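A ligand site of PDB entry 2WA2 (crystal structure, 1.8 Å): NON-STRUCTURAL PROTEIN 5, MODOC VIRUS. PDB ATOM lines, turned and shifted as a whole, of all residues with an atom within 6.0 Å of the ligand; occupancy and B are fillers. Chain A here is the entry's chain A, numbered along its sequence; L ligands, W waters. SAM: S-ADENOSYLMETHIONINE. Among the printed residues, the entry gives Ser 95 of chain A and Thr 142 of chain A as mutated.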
ATOM      1  N   SER A  65      -7.356  14.721  15.030  1.00  0.00           N
ATOM      2  CA  SER A  65      -6.946  13.765  16.053  1.00  0.00           C
ATOM      3  C   SER A  65      -6.129  14.444  17.175  1.00  0.00           C
ATOM      4  O   SER A  65      -5.336  15.346  16.917  1.00  0.00           O
ATOM      5  CB  SER A  65      -6.106  12.663  15.397  1.00  0.00           C
ATOM      6  OG  SER A  65      -5.415  11.874  16.334  1.00  0.00           O
ATOM      7  N   GLY A  67      -3.832  12.912  18.758  1.00  0.00           N
ATOM      8  CA  GLY A  67      -2.480  12.393  18.447  1.00  0.00           C
ATOM      9  C   GLY A  67      -1.809  13.266  17.410  1.00  0.00           C
ATOM     10  O   GLY A  67      -0.648  13.652  17.573  1.00  0.00           O
ATOM     11  N   THR A  68      -2.549  13.595  16.358  1.00  0.00           N
ATOM     12  CA  THR A  68      -2.039  14.464  15.316  1.00  0.00           C
ATOM     13  C   THR A  68      -1.640  15.821  15.892  1.00  0.00           C
ATOM     14  O   THR A  68      -0.545  16.310  15.636  1.00  0.00           O
ATOM     15  CB  THR A  68      -3.070  14.658  14.191  1.00  0.00           C
ATOM     16  OG1 THR A  68      -3.286  13.390  13.560  1.00  0.00           O
ATOM     17  CG2 THR A  68      -2.593  15.657  13.145  1.00  0.00           C
ATOM     18  N   ASP A  88       7.379   4.248  13.874  1.00  0.00           N
ATOM     19  CA  ASP A  88       6.327   4.672  14.772  1.00  0.00           C
ATOM     20  C   ASP A  88       5.977   3.452  15.614  1.00  0.00           C
ATOM     21  O   ASP A  88       5.261   2.550  15.167  1.00  0.00           O
ATOM     22  CB  ASP A  88       5.134   5.234  13.995  1.00  0.00           C
ATOM     23  CG  ASP A  88       4.040   5.786  14.906  1.00  0.00           C
ATOM     24  OD1 ASP A  88       4.271   5.894  16.132  1.00  0.00           O
ATOM     25  OD2 ASP A  88       2.929   6.058  14.413  1.00  0.00           O
ATOM     26  N   LEU A  89       6.550   3.415  16.811  1.00  0.00           N
ATOM     27  CA  LEU A  89       6.341   2.312  17.737  1.00  0.00           C
ATOM     28  C   LEU A  89       5.114   2.532  18.604  1.00  0.00           C
ATOM     29  O   LEU A  89       4.986   3.569  19.271  1.00  0.00           O
ATOM     30  CB  LEU A  89       7.604   2.092  18.595  1.00  0.00           C
ATOM     31  CG  LEU A  89       8.869   1.894  17.739  1.00  0.00           C
ATOM     32  CD1 LEU A  89      10.092   1.983  18.607  1.00  0.00           C
ATOM     33  CD2 LEU A  89       8.868   0.561  16.931  1.00  0.00           C
ATOM     34  N   GLY A  90       4.191   1.577  18.564  1.00  0.00           N
ATOM     35  CA  GLY A  90       2.921   1.736  19.278  1.00  0.00           C
ATOM     36  C   GLY A  90       2.036   2.703  18.508  1.00  0.00           C
ATOM     37  O   GLY A  90       1.609   3.710  19.029  1.00  0.00           O
ATOM     38  N   CYS A  91       1.808   2.407  17.230  1.00  0.00           N
ATOM     39  CA  CYS A  91       1.142   3.383  16.370  1.00  0.00           C
ATOM     40  C   CYS A  91      -0.362   3.479  16.618  1.00  0.00           C
ATOM     41  O   CYS A  91      -0.994   4.497  16.254  1.00  0.00           O
ATOM     42  CB  CYS A  91       1.478   3.103  14.889  1.00  0.00           C
ATOM     43  SG  CYS A  91       0.627   1.664  14.184  1.00  0.00           S
ATOM     44  N   GLY A  92      -0.952   2.458  17.231  1.00  0.00           N
ATOM     45  CA  GLY A  92      -2.403   2.420  17.403  1.00  0.00           C
ATOM     46  C   GLY A  92      -3.119   2.700  16.098  1.00  0.00           C
ATOM     47  O   GLY A  92      -2.790   2.085  15.056  1.00  0.00           O
ATOM     48  N   ARG A  93      -4.053   3.652  16.125  1.00  0.00           N
ATOM     49  CA  ARG A  93      -4.802   4.027  14.904  1.00  0.00           C
ATOM     50  C   ARG A  93      -3.889   4.598  13.828  1.00  0.00           C
ATOM     51  O   ARG A  93      -4.191   4.548  12.649  1.00  0.00           O
ATOM     52  CB  ARG A  93      -5.928   5.007  15.230  1.00  0.00           C
ATOM     53  CG  ARG A  93      -6.944   4.420  16.184  1.00  0.00           C
ATOM     54  CD  ARG A  93      -8.138   5.349  16.459  1.00  0.00           C
ATOM     55  NE  ARG A  93      -8.941   4.853  17.589  1.00  0.00           N
ATOM     56  CZ  ARG A  93     -10.054   5.425  18.040  1.00  0.00           C
ATOM     57  NH1 ARG A  93     -10.530   6.532  17.472  1.00  0.00           N
ATOM     58  NH2 ARG A  93     -10.708   4.894  19.074  1.00  0.00           N
ATOM     59  N   GLY A  94      -2.749   5.148  14.222  1.00  0.00           N
ATOM     60  CA  GLY A  94      -1.773   5.589  13.234  1.00  0.00           C
ATOM     61  C   GLY A  94      -1.727   7.076  12.894  1.00  0.00           C
ATOM     62  O   GLY A  94      -1.188   7.445  11.852  1.00  0.00           O
ATOM     63  N   SER A  95      -2.245   7.931  13.782  1.00  0.00           N
ATOM     64  CA  SER A  95      -2.259   9.393  13.533  1.00  0.00           C
ATOM     65  C   SER A  95      -0.857   9.949  13.409  1.00  0.00           C
ATOM     66  O   SER A  95      -0.615  10.799  12.554  1.00  0.00           O
ATOM     67  CB  SER A  95      -3.024  10.162  14.625  1.00  0.00           C
ATOM     68  OG  SER A  95      -4.417  10.059  14.413  1.00  0.00           O
ATOM     69  N   TRP A  96       0.075   9.499  14.243  1.00  0.00           N
ATOM     70  CA  TRP A  96       1.461   9.972  14.136  1.00  0.00           C
ATOM     71  C   TRP A  96       2.087   9.568  12.805  1.00  0.00           C
ATOM     72  O   TRP A  96       2.876  10.299  12.245  1.00  0.00           O
ATOM     73  CB  TRP A  96       2.326   9.433  15.300  1.00  0.00           C
ATOM     74  CG  TRP A  96       2.176  10.227  16.622  1.00  0.00           C
ATOM     75  CD1 TRP A  96       1.137  11.045  16.989  1.00  0.00           C
ATOM     76  CD2 TRP A  96       3.119  10.274  17.692  1.00  0.00           C
ATOM     77  NE1 TRP A  96       1.380  11.596  18.242  1.00  0.00           N
ATOM     78  CE2 TRP A  96       2.587  11.128  18.697  1.00  0.00           C
ATOM     79  CE3 TRP A  96       4.383   9.670  17.914  1.00  0.00           C
ATOM     80  CZ2 TRP A  96       3.274  11.418  19.884  1.00  0.00           C
ATOM     81  CZ3 TRP A  96       5.070   9.968  19.113  1.00  0.00           C
ATOM     82  CH2 TRP A  96       4.503  10.821  20.078  1.00  0.00           C
ATOM     83  N   SER A  97       1.755   8.378  12.325  1.00  0.00           N
ATOM     84  CA  SER A  97       2.338   7.850  11.095  1.00  0.00           C
ATOM     85  C   SER A  97       1.862   8.660   9.888  1.00  0.00           C
ATOM     86  O   SER A  97       2.664   8.978   9.000  1.00  0.00           O
ATOM     87  CB  SER A  97       1.962   6.374  10.949  1.00  0.00           C
ATOM     88  OG  SER A  97       2.798   5.607  11.804  1.00  0.00           O
ATOM     89  N   TYR A 112       4.163   0.211  13.828  1.00  0.00           N
ATOM     90  CA  TYR A 112       3.995  -1.066  14.521  1.00  0.00           C
ATOM     91  C   TYR A 112       3.079  -0.920  15.722  1.00  0.00           C
ATOM     92  O   TYR A 112       3.198   0.047  16.488  1.00  0.00           O
ATOM     93  CB  TYR A 112       5.373  -1.607  14.978  1.00  0.00           C
ATOM     94  CG  TYR A 112       6.319  -1.811  13.820  1.00  0.00           C
ATOM     95  CD1 TYR A 112       6.324  -3.019  13.118  1.00  0.00           C
ATOM     96  CD2 TYR A 112       7.194  -0.792  13.423  1.00  0.00           C
ATOM     97  CE1 TYR A 112       7.192  -3.203  12.023  1.00  0.00           C
ATOM     98  CE2 TYR A 112       8.078  -0.972  12.326  1.00  0.00           C
ATOM     99  CZ  TYR A 112       8.059  -2.163  11.646  1.00  0.00           C
ATOM    100  OH  TYR A 112       8.911  -2.372  10.575  1.00  0.00           O
ATOM    101  N   THR A 113       2.154  -1.866  15.909  1.00  0.00           N
ATOM    102  CA  THR A 113       1.312  -1.827  17.092  1.00  0.00           C
ATOM    103  C   THR A 113       0.769  -3.218  17.433  1.00  0.00           C
ATOM    104  O   THR A 113       0.749  -4.122  16.578  1.00  0.00           O
ATOM    105  CB  THR A 113       0.178  -0.769  16.914  1.00  0.00           C
ATOM    106  OG1 THR A 113      -0.269  -0.305  18.208  1.00  0.00           O
ATOM    107  CG2 THR A 113      -0.969  -1.276  16.045  1.00  0.00           C
ATOM    108  N   LEU A 114       0.388  -3.406  18.687  1.00  0.00           N
ATOM    109  CA  LEU A 114      -0.131  -4.681  19.165  1.00  0.00           C
ATOM    110  C   LEU A 114      -1.404  -5.083  18.398  1.00  0.00           C
ATOM    111  O   LEU A 114      -1.455  -6.149  17.816  1.00  0.00           O
ATOM    112  CB  LEU A 114      -0.457  -4.595  20.632  1.00  0.00           C
ATOM    113  CG  LEU A 114       0.527  -5.038  21.686  1.00  0.00           C
ATOM    114  CD1 LEU A 114      -0.264  -5.059  22.981  1.00  0.00           C
ATOM    115  CD2 LEU A 114       1.116  -6.435  21.403  1.00  0.00           C
ATOM    116  N   GLY A 115      -2.420  -4.221  18.431  1.00  0.00           N
ATOM    117  CA  GLY A 115      -3.619  -4.392  17.613  1.00  0.00           C
ATOM    118  C   GLY A 115      -4.391  -5.649  18.006  1.00  0.00           C
ATOM    119  O   GLY A 115      -5.220  -6.123  17.248  1.00  0.00           O
ATOM    120  N   HIS A 119      -7.119  -3.405  21.763  1.00  0.00           N
ATOM    121  CA  HIS A 119      -6.045  -2.473  21.426  1.00  0.00           C
ATOM    122  C   HIS A 119      -6.356  -1.891  20.067  1.00  0.00           C
ATOM    123  O   HIS A 119      -6.822  -2.601  19.170  1.00  0.00           O
ATOM    124  CB  HIS A 119      -4.689  -3.162  21.361  1.00  0.00           C
ATOM    125  CG  HIS A 119      -4.108  -3.521  22.689  1.00  0.00           C
ATOM    126  ND1 HIS A 119      -3.130  -2.772  23.302  1.00  0.00           N
ATOM    127  CD2 HIS A 119      -4.329  -4.585  23.500  1.00  0.00           C
ATOM    128  CE1 HIS A 119      -2.799  -3.331  24.448  1.00  0.00           C
ATOM    129  NE2 HIS A 119      -3.502  -4.446  24.597  1.00  0.00           N
ATOM    130  N   GLU A 120      -6.085  -0.599  19.904  1.00  0.00           N
ATOM    131  CA  GLU A 120      -6.346   0.096  18.650  1.00  0.00           C
ATOM    132  C   GLU A 120      -5.595  -0.540  17.485  1.00  0.00           C
ATOM    133  O   GLU A 120      -4.408  -0.843  17.606  1.00  0.00           O
ATOM    134  CB  GLU A 120      -5.943   1.578  18.743  1.00  0.00           C
ATOM    135  CG  GLU A 120      -6.656   2.373  19.819  1.00  0.00           C
ATOM    136  CD  GLU A 120      -8.161   2.333  19.668  1.00  0.00           C
ATOM    137  OE1 GLU A 120      -8.638   2.413  18.502  1.00  0.00           O
ATOM    138  OE2 GLU A 120      -8.870   2.232  20.705  1.00  0.00           O
ATOM    139  N   VAL A 139       2.297  -7.017  16.611  1.00  0.00           N
ATOM    140  CA  VAL A 139       3.714  -6.944  16.957  1.00  0.00           C
ATOM    141  C   VAL A 139       3.836  -6.301  18.337  1.00  0.00           C
ATOM    142  O   VAL A 139       3.229  -5.234  18.590  1.00  0.00           O
ATOM    143  CB  VAL A 139       4.543  -6.087  15.921  1.00  0.00           C
ATOM    144  CG1 VAL A 139       5.945  -5.885  16.395  1.00  0.00           C
ATOM    145  CG2 VAL A 139       4.589  -6.781  14.554  1.00  0.00           C
ATOM    146  N   ASP A 140       4.593  -6.975  19.194  1.00  0.00           N
ATOM    147  CA  ASP A 140       4.958  -6.455  20.507  1.00  0.00           C
ATOM    148  C   ASP A 140       6.295  -5.733  20.298  1.00  0.00           C
ATOM    149  O   ASP A 140       7.340  -6.374  20.121  1.00  0.00           O
ATOM    150  CB  ASP A 140       5.119  -7.594  21.520  1.00  0.00           C
ATOM    151  CG  ASP A 140       5.511  -7.096  22.913  1.00  0.00           C
ATOM    152  OD1 ASP A 140       5.838  -5.882  23.088  1.00  0.00           O
ATOM    153  OD2 ASP A 140       5.492  -7.949  23.826  1.00  0.00           O
ATOM    154  N   VAL A 141       6.253  -4.412  20.326  1.00  0.00           N
ATOM    155  CA  VAL A 141       7.444  -3.636  20.001  1.00  0.00           C
ATOM    156  C   VAL A 141       8.508  -3.766  21.070  1.00  0.00           C
ATOM    157  O   VAL A 141       9.672  -3.544  20.779  1.00  0.00           O
ATOM    158  CB  VAL A 141       7.166  -2.137  19.697  1.00  0.00           C
ATOM    159  CG1 VAL A 141       6.142  -1.963  18.551  1.00  0.00           C
ATOM    160  CG2 VAL A 141       6.763  -1.404  20.951  1.00  0.00           C
ATOM    161  N   THR A 142       8.150  -4.137  22.295  1.00  0.00           N
ATOM    162  CA  THR A 142       9.155  -4.352  23.326  1.00  0.00           C
ATOM    163  C   THR A 142      10.078  -5.541  23.021  1.00  0.00           C
ATOM    164  O   THR A 142      11.115  -5.718  23.688  1.00  0.00           O
ATOM    165  CB  THR A 142       8.569  -4.531  24.757  1.00  0.00           C
ATOM    166  OG1 THR A 142       7.929  -5.815  24.843  1.00  0.00           O
ATOM    167  CG2 THR A 142       7.584  -3.405  25.126  1.00  0.00           C
ATOM    168  N   ASP A 155       4.691   6.377  21.076  1.00  0.00           N
ATOM    169  CA  ASP A 155       3.635   7.023  21.847  1.00  0.00           C
ATOM    170  C   ASP A 155       2.913   5.977  22.716  1.00  0.00           C
ATOM    171  O   ASP A 155       1.698   5.996  22.869  1.00  0.00           O
ATOM    172  CB  ASP A 155       2.682   7.749  20.893  1.00  0.00           C
ATOM    173  CG  ASP A 155       1.777   8.780  21.576  1.00  0.00           C
ATOM    174  OD1 ASP A 155       2.136   9.339  22.641  1.00  0.00           O
ATOM    175  OD2 ASP A 155       0.703   9.066  21.025  1.00  0.00           O
ATOM    176  N   ILE A 156       3.688   5.064  23.288  1.00  0.00           N
ATOM    177  CA  ILE A 156       3.142   4.034  24.172  1.00  0.00           C
ATOM    178  C   ILE A 156       3.013   4.560  25.625  1.00  0.00           C
ATOM    179  O   ILE A 156       3.914   5.212  26.133  1.00  0.00           O
ATOM    180  CB  ILE A 156       4.025   2.761  24.143  1.00  0.00           C
ATOM    181  CG1 ILE A 156       4.000   2.131  22.746  1.00  0.00           C
ATOM    182  CG2 ILE A 156       3.603   1.730  25.192  1.00  0.00           C
ATOM    183  CD1 ILE A 156       4.920   0.973  22.647  1.00  0.00           C
ATOM    184  N   GLY A 157       1.891   4.250  26.269  1.00  0.00           N
ATOM    185  CA  GLY A 157       1.708   4.554  27.684  1.00  0.00           C
ATOM    186  C   GLY A 157       0.238   4.787  27.873  1.00  0.00           C
ATOM    187  O   GLY A 157      -0.299   5.810  27.423  1.00  0.00           O
HETATM  188  N   SAM L   1       0.339   7.966  18.458  1.00  0.00           N
HETATM  189  CA  SAM L   1      -0.986   7.266  18.438  1.00  0.00           C
HETATM  190  C   SAM L   1      -1.929   7.935  17.428  1.00  0.00           C
HETATM  191  O   SAM L   1      -1.634   9.048  16.976  1.00  0.00           O
HETATM  192  OXT SAM L   1      -2.993   7.409  17.051  1.00  0.00           O
HETATM  193  CB  SAM L   1      -1.613   7.295  19.834  1.00  0.00           C
HETATM  194  CG  SAM L   1      -0.910   6.408  20.847  1.00  0.00           C
HETATM  195  SD  SAM L   1      -1.571   4.741  20.670  1.00  0.00           S
HETATM  196  CE  SAM L   1      -3.000   4.893  21.787  1.00  0.00           C
HETATM  197  C5' SAM L   1      -0.505   3.766  21.760  1.00  0.00           C
HETATM  198  C4' SAM L   1      -0.582   2.334  21.253  1.00  0.00           C
HETATM  199  O4' SAM L   1       0.521   1.568  21.659  1.00  0.00           O
HETATM  200  C3' SAM L   1      -1.811   1.610  21.778  1.00  0.00           C
HETATM  201  O3' SAM L   1      -2.709   1.464  20.711  1.00  0.00           O
HETATM  202  C2' SAM L   1      -1.319   0.245  22.239  1.00  0.00           C
HETATM  203  O2' SAM L   1      -2.116  -0.770  21.671  1.00  0.00           O
HETATM  204  C1' SAM L   1       0.104   0.214  21.661  1.00  0.00           C
HETATM  205  N9  SAM L   1       1.019  -0.616  22.439  1.00  0.00           N
HETATM  206  C8  SAM L   1       1.115  -0.680  23.805  1.00  0.00           C
HETATM  207  N7  SAM L   1       2.085  -1.547  24.132  1.00  0.00           N
HETATM  208  C5  SAM L   1       2.586  -2.041  22.964  1.00  0.00           C
HETATM  209  C6  SAM L   1       3.591  -2.966  22.705  1.00  0.00           C
HETATM  210  N6  SAM L   1       4.254  -3.580  23.667  1.00  0.00           N
HETATM  211  N1  SAM L   1       3.907  -3.248  21.383  1.00  0.00           N
HETATM  212  C2  SAM L   1       3.233  -2.652  20.358  1.00  0.00           C
HETATM  213  N3  SAM L   1       2.230  -1.719  20.596  1.00  0.00           N
HETATM  214  C4  SAM L   1       1.926  -1.450  21.900  1.00  0.00           C
HETATM  215  O   HOH W   1       3.970  -3.578  26.346  1.00  0.00           O
HETATM  216  O   HOH W   2      -2.416  -1.412  19.272  1.00  0.00           O
HETATM  217  O   HOH W   3       2.361   6.270  17.870  1.00  0.00           O
HETATM  218  O   HOH W   4      -5.180   1.170  22.365  1.00  0.00           O
HETATM  219  O   HOH W   5      -4.286   5.214  18.429  1.00  0.00           O
HETATM  220  O   HOH W   6      -0.149   2.725  25.042  1.00  0.00           O
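ND1 of His 119 is in hydrogen-bond range of O2' of the ligand. N of Trp 96 is in hydrogen-bond range of O of the ligand. N of Val 141 lies within hydrogen-bond range of N1 of the ligand, at 2.8 Å. An oxygen (OXT) of the ligand is in hydrogen-bond range of the backbone NH (N) of Ser 95, 3.4 Å away. A nitrogen (N) of the ligand lies within salt-bridge range of the side-chain carboxylate of Asp 155 (2.8 Å). The side-chain carboxylate of Asp 140 is in hydrogen-bond range of a nitrogen (N6) of the ligand (2.9 Å). A nitrogen (N3) of the ligand lies within hydrogen-bond range of the backbone NH of Leu 114.
A sulfur (SD) of the ligand sits close to the backbone carbonyl oxygen (O) of Gly 90, 3.7 Å away. The backbone carbonyl oxygen (O) of Val 139 sits close to a nitrogen (N1) of the ligand (3.5 Å). Gly 67 touches the ligand (CA to O, 3.8 Å). Cys 91 touches the ligand (O to CA, 3.5 Å). Gly 92 touches the ligand. Gly 94 touches the ligand (N to OXT, 3.6 Å). Thr 113 touches the ligand. Glu 120 touches the ligand (CB to O3', 3.8 Å). CG2 of Thr 142 touches N6 of the ligand, at 3.6 Å. Ile 156 touches the ligand. Hydrophobic or aromatic side chains that line the ligand: Trp 96, Leu 114, His 119, Val 141 and Ile 156. 17 residues have an atom within 4 Å of the ligand: Gly 67, Gly 90, Cys 91, Gly 92, Gly 94, Ser 95, Trp 96, Thr 113, Leu 114, His 119, Glu 120, Val 139, Asp 140, Val 141, Thr 142, Asp 155 and Ile 156.
Water W2 lies within hydrogen-bond range of O2' of the ligand (2.5 Å), OG1 of Thr 113 (2.6 Å), O of Glu 120 (2.7 Å), N of Gly 115 (2.9 Å) and N of Leu 114 (3.5 Å). Water W3 lies within hydrogen-bond range of the side-chain carboxylate (OD1) of Asp 88 (2.6 Å), a nitrogen (N) of the ligand (2.7 Å) and the backbone carbonyl oxygen (O) of Gly 90 (2.9 Å). Water W5 bridges N of Arg 93 (2.8 Å) and OXT of the ligand (2.9 Å). Water W4 bridges O3' of the ligand (3.0 Å) and N of Glu 120 (3.2 Å).
The side-chain hydroxyl (OG1) of Thr 142 is in hydrogen-bond range of the side-chain carboxylate (OD1) of Asp 140 (2.7 Å). O of Gly 67 sits at hydrogen-bond distance from NE1 of Trp 96, 3.0 Å away. O of Val 139 lies within hydrogen-bond range of N of Leu 114. N of Asp 155 is in hydrogen-bond range of O of Leu 89. OE1 of Glu 120 is in salt-bridge range of NE of Arg 93 (2.6 Å). N of Gly 67 sits at hydrogen-bond distance from OG of Ser 65, at 3.1 Å. The backbone NH of Val 139 sits at hydrogen-bond distance from the backbone carbonyl oxygen of Thr 113. The backbone NH (N) of Gly 92 is in hydrogen-bond range of the side-chain hydroxyl (OG1) of Thr 113.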
